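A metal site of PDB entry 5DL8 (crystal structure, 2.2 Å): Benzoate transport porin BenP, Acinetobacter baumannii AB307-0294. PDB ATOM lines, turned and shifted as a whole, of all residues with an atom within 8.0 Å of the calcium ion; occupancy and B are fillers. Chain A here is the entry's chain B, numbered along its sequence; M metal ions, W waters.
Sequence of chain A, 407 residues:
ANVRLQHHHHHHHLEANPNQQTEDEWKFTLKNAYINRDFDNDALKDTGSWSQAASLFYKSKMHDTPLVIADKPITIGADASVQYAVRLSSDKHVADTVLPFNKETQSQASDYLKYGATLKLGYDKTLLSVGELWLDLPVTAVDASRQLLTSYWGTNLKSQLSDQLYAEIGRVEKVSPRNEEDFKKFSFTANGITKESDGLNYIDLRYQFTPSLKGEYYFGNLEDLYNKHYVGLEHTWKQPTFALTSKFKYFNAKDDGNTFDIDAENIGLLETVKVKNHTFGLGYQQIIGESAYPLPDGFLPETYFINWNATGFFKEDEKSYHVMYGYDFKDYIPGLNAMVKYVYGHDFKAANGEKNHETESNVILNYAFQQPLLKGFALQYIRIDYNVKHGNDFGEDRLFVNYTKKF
N of Asp 38 sits at hydrogen-bond distance from O of Gly 395.
Of the 15 residues printed, 3 come within 4 Å of the calcium ion.
The nearest printed residue that does not touch the calcium ion is Asn 41 (4.7 Å).
The calcium ion is bound by water W2, water W1, the side-chain carboxylate (OD1) of Asp 46, water W4, the side-chain carboxylate (OD1) of Asp 38, water W3, the backbone carbonyl oxygen (O) of Phe 39 and the side-chain carboxylate (OD2) of Asp 46.
The calcium ion has eight donor atoms within binding distance.
Water W2 lies within hydrogen-bond range of the side-chain carboxylate of Asp 42 (3.1 Å) and the backbone carbonyl oxygen of Asp 40 (3.4 Å).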
ATOM      1  N   ASN A  36     -27.736   1.876  22.969  1.00  0.00           N
ATOM      2  CA  ASN A  36     -26.282   2.046  22.895  1.00  0.00           C
ATOM      3  C   ASN A  36     -25.782   2.690  24.154  1.00  0.00           C
ATOM      4  O   ASN A  36     -26.087   3.855  24.424  1.00  0.00           O
ATOM      5  CB  ASN A  36     -25.821   2.873  21.619  1.00  0.00           C
ATOM      6  CG  ASN A  36     -24.374   2.639  21.264  1.00  0.00           C
ATOM      7  OD1 ASN A  36     -23.997   1.547  20.781  1.00  0.00           O
ATOM      8  ND2 ASN A  36     -23.564   3.618  21.500  1.00  0.00           N
ATOM      9  N   ARG A  37     -25.018   1.943  24.945  1.00  0.00           N
ATOM     10  CA  ARG A  37     -24.327   2.541  26.103  1.00  0.00           C
ATOM     11  C   ARG A  37     -22.862   2.734  25.803  1.00  0.00           C
ATOM     12  O   ARG A  37     -22.133   1.800  25.649  1.00  0.00           O
ATOM     13  CB  ARG A  37     -24.526   1.690  27.391  1.00  0.00           C
ATOM     14  CG  ARG A  37     -23.837   2.251  28.665  1.00  0.00           C
ATOM     15  CD  ARG A  37     -24.287   1.546  29.969  1.00  0.00           C
ATOM     16  NE  ARG A  37     -25.656   1.759  30.285  1.00  0.00           N
ATOM     17  CZ  ARG A  37     -26.291   1.382  31.427  1.00  0.00           C
ATOM     18  NH1 ARG A  37     -25.673   0.721  32.392  1.00  0.00           N
ATOM     19  NH2 ARG A  37     -27.617   1.685  31.574  1.00  0.00           N
ATOM     20  N   ASP A  38     -22.424   3.969  25.871  1.00  0.00           N
ATOM     21  CA  ASP A  38     -21.064   4.356  25.501  1.00  0.00           C
ATOM     22  C   ASP A  38     -20.335   4.893  26.714  1.00  0.00           C
ATOM     23  O   ASP A  38     -20.611   6.034  27.170  1.00  0.00           O
ATOM     24  CB  ASP A  38     -21.161   5.483  24.407  1.00  0.00           C
ATOM     25  CG  ASP A  38     -19.785   6.013  23.940  1.00  0.00           C
ATOM     26  OD1 ASP A  38     -18.805   5.927  24.705  1.00  0.00           O
ATOM     27  OD2 ASP A  38     -19.682   6.561  22.818  1.00  0.00           O
ATOM     28  N   PHE A  39     -19.383   4.127  27.226  1.00  0.00           N
ATOM     29  CA  PHE A  39     -18.445   4.615  28.271  1.00  0.00           C
ATOM     30  C   PHE A  39     -17.499   5.735  27.810  1.00  0.00           C
ATOM     31  O   PHE A  39     -16.915   5.664  26.791  1.00  0.00           O
ATOM     32  CB  PHE A  39     -17.753   3.436  28.940  1.00  0.00           C
ATOM     33  CG  PHE A  39     -18.741   2.465  29.537  1.00  0.00           C
ATOM     34  CD1 PHE A  39     -19.294   2.672  30.828  1.00  0.00           C
ATOM     35  CD2 PHE A  39     -19.127   1.355  28.896  1.00  0.00           C
ATOM     36  CE1 PHE A  39     -20.206   1.763  31.381  1.00  0.00           C
ATOM     37  CE2 PHE A  39     -19.993   0.418  29.443  1.00  0.00           C
ATOM     38  CZ  PHE A  39     -20.580   0.642  30.671  1.00  0.00           C
ATOM     39  N   ASP A  40     -17.411   6.834  28.577  1.00  0.00           N
ATOM     40  CA  ASP A  40     -16.426   7.874  28.328  1.00  0.00           C
ATOM     41  C   ASP A  40     -14.976   7.310  28.292  1.00  0.00           C
ATOM     42  O   ASP A  40     -14.157   7.663  27.441  1.00  0.00           O
ATOM     43  CB  ASP A  40     -16.526   8.946  29.408  1.00  0.00           C
ATOM     44  CG  ASP A  40     -17.775   9.795  29.298  1.00  0.00           C
ATOM     45  OD1 ASP A  40     -18.810   9.398  28.782  1.00  0.00           O
ATOM     46  OD2 ASP A  40     -17.763  10.890  29.753  1.00  0.00           O
ATOM     47  N   ASN A  41     -14.657   6.447  29.247  1.00  0.00           N
ATOM     48  CA  ASN A  41     -13.341   5.836  29.301  1.00  0.00           C
ATOM     49  C   ASN A  41     -13.107   4.797  28.132  1.00  0.00           C
ATOM     50  O   ASN A  41     -13.848   3.746  28.002  1.00  0.00           O
ATOM     51  CB  ASN A  41     -13.172   5.257  30.687  1.00  0.00           C
ATOM     52  CG  ASN A  41     -11.852   4.551  30.924  1.00  0.00           C
ATOM     53  OD1 ASN A  41     -10.954   4.481  30.096  1.00  0.00           O
ATOM     54  ND2 ASN A  41     -11.736   4.032  32.126  1.00  0.00           N
ATOM     55  N   ASP A  42     -12.096   5.110  27.284  1.00  0.00           N
ATOM     56  CA  ASP A  42     -11.681   4.277  26.102  1.00  0.00           C
ATOM     57  C   ASP A  42     -11.308   2.850  26.467  1.00  0.00           C
ATOM     58  O   ASP A  42     -11.451   1.986  25.610  1.00  0.00           O
ATOM     59  CB  ASP A  42     -10.465   4.889  25.358  1.00  0.00           C
ATOM     60  CG  ASP A  42     -10.793   6.177  24.659  1.00  0.00           C
ATOM     61  OD1 ASP A  42     -11.945   6.391  24.318  1.00  0.00           O
ATOM     62  OD2 ASP A  42      -9.914   7.005  24.445  1.00  0.00           O
ATOM     63  N   ALA A  43     -10.798   2.621  27.701  1.00  0.00           N
ATOM     64  CA  ALA A  43     -10.451   1.298  28.147  1.00  0.00           C
ATOM     65  C   ALA A  43     -11.632   0.377  28.294  1.00  0.00           C
ATOM     66  O   ALA A  43     -11.416  -0.814  28.353  1.00  0.00           O
ATOM     67  CB  ALA A  43      -9.692   1.337  29.436  1.00  0.00           C
ATOM     68  N   LEU A  44     -12.861   0.913  28.413  1.00  0.00           N
ATOM     69  CA  LEU A  44     -14.035   0.064  28.579  1.00  0.00           C
ATOM     70  C   LEU A  44     -14.757  -0.182  27.258  1.00  0.00           C
ATOM     71  O   LEU A  44     -14.757   0.661  26.373  1.00  0.00           O
ATOM     72  CB  LEU A  44     -15.009   0.670  29.627  1.00  0.00           C
ATOM     73  CG  LEU A  44     -14.432   1.108  31.001  1.00  0.00           C
ATOM     74  CD1 LEU A  44     -15.504   1.787  31.863  1.00  0.00           C
ATOM     75  CD2 LEU A  44     -13.763  -0.016  31.775  1.00  0.00           C
ATOM     76  N   LYS A  45     -15.470  -1.300  27.192  1.00  0.00           N
ATOM     77  CA  LYS A  45     -16.259  -1.657  26.046  1.00  0.00           C
ATOM     78  C   LYS A  45     -17.721  -1.237  26.034  1.00  0.00           C
ATOM     79  O   LYS A  45     -18.514  -1.609  26.925  1.00  0.00           O
ATOM     80  CB  LYS A  45     -16.225  -3.168  25.864  1.00  0.00           C
ATOM     81  CG  LYS A  45     -16.463  -3.642  24.410  1.00  0.00           C
ATOM     82  CD  LYS A  45     -16.170  -5.129  24.216  1.00  0.00           C
ATOM     83  CE  LYS A  45     -14.954  -5.584  25.044  1.00  0.00           C
ATOM     84  NZ  LYS A  45     -14.542  -7.014  24.838  1.00  0.00           N
ATOM     85  N   ASP A  46     -18.071  -0.552  24.945  1.00  0.00           N
ATOM     86  CA  ASP A  46     -19.418  -0.032  24.669  1.00  0.00           C
ATOM     87  C   ASP A  46     -20.407  -1.189  24.487  1.00  0.00           C
ATOM     88  O   ASP A  46     -20.039  -2.211  23.977  1.00  0.00           O
ATOM     89  CB  ASP A  46     -19.376   0.856  23.440  1.00  0.00           C
ATOM     90  CG  ASP A  46     -18.641   2.190  23.698  1.00  0.00           C
ATOM     91  OD1 ASP A  46     -18.214   2.573  24.877  1.00  0.00           O
ATOM     92  OD2 ASP A  46     -18.567   2.943  22.713  1.00  0.00           O
ATOM     93  N   THR A  47     -21.643  -1.090  25.022  1.00  0.00           N
ATOM     94  CA  THR A  47     -22.585  -2.167  24.848  1.00  0.00           C
ATOM     95  C   THR A  47     -23.838  -1.677  24.152  1.00  0.00           C
ATOM     96  O   THR A  47     -24.106  -0.462  24.015  1.00  0.00           O
ATOM     97  CB  THR A  47     -22.978  -2.690  26.221  1.00  0.00           C
ATOM     98  OG1 THR A  47     -23.768  -1.685  26.905  1.00  0.00           O
ATOM     99  CG2 THR A  47     -21.717  -3.075  27.037  1.00  0.00           C
ATOM    100  N   ASP A 393     -18.127   6.807  33.835  1.00  0.00           N
ATOM    101  CA  ASP A 393     -19.090   7.738  33.239  1.00  0.00           C
ATOM    102  C   ASP A 393     -19.640   7.135  31.943  1.00  0.00           C
ATOM    103  O   ASP A 393     -18.912   6.380  31.322  1.00  0.00           O
ATOM    104  CB  ASP A 393     -18.471   9.066  32.905  1.00  0.00           C
ATOM    105  CG  ASP A 393     -18.009   9.812  34.106  1.00  0.00           C
ATOM    106  OD1 ASP A 393     -18.256   9.397  35.233  1.00  0.00           O
ATOM    107  OD2 ASP A 393     -17.382  10.866  33.934  1.00  0.00           O
ATOM    108  N   PHE A 394     -20.923   7.375  31.596  1.00  0.00           N
ATOM    109  CA  PHE A 394     -21.405   6.971  30.298  1.00  0.00           C
ATOM    110  C   PHE A 394     -22.568   7.828  29.692  1.00  0.00           C
ATOM    111  O   PHE A 394     -23.272   8.573  30.383  1.00  0.00           O
ATOM    112  CB  PHE A 394     -21.780   5.502  30.344  1.00  0.00           C
ATOM    113  CG  PHE A 394     -23.038   5.211  31.132  1.00  0.00           C
ATOM    114  CD1 PHE A 394     -24.299   5.419  30.574  1.00  0.00           C
ATOM    115  CD2 PHE A 394     -22.956   4.658  32.379  1.00  0.00           C
ATOM    116  CE1 PHE A 394     -25.457   5.123  31.266  1.00  0.00           C
ATOM    117  CE2 PHE A 394     -24.108   4.365  33.103  1.00  0.00           C
ATOM    118  CZ  PHE A 394     -25.370   4.601  32.544  1.00  0.00           C
ATOM    119  N   GLY A 395     -22.725   7.690  28.388  1.00  0.00           N
ATOM    120  CA  GLY A 395     -23.873   8.234  27.625  1.00  0.00           C
ATOM    121  C   GLY A 395     -24.575   7.116  26.907  1.00  0.00           C
ATOM    122  O   GLY A 395     -23.950   6.362  26.206  1.00  0.00           O
HETATM  123 CA    CA M   1     -16.833   4.438  24.467  1.00  0.00          CA
HETATM  124  O   HOH W   1     -16.725   6.105  22.841  1.00  0.00           O
HETATM  125  O   HOH W   2     -15.009   5.850  24.733  1.00  0.00           O
HETATM  126  O   HOH W   3     -15.021   3.329  23.095  1.00  0.00           O
HETATM  127  O   HOH W   4     -15.473   3.127  25.921  1.00  0.00           O
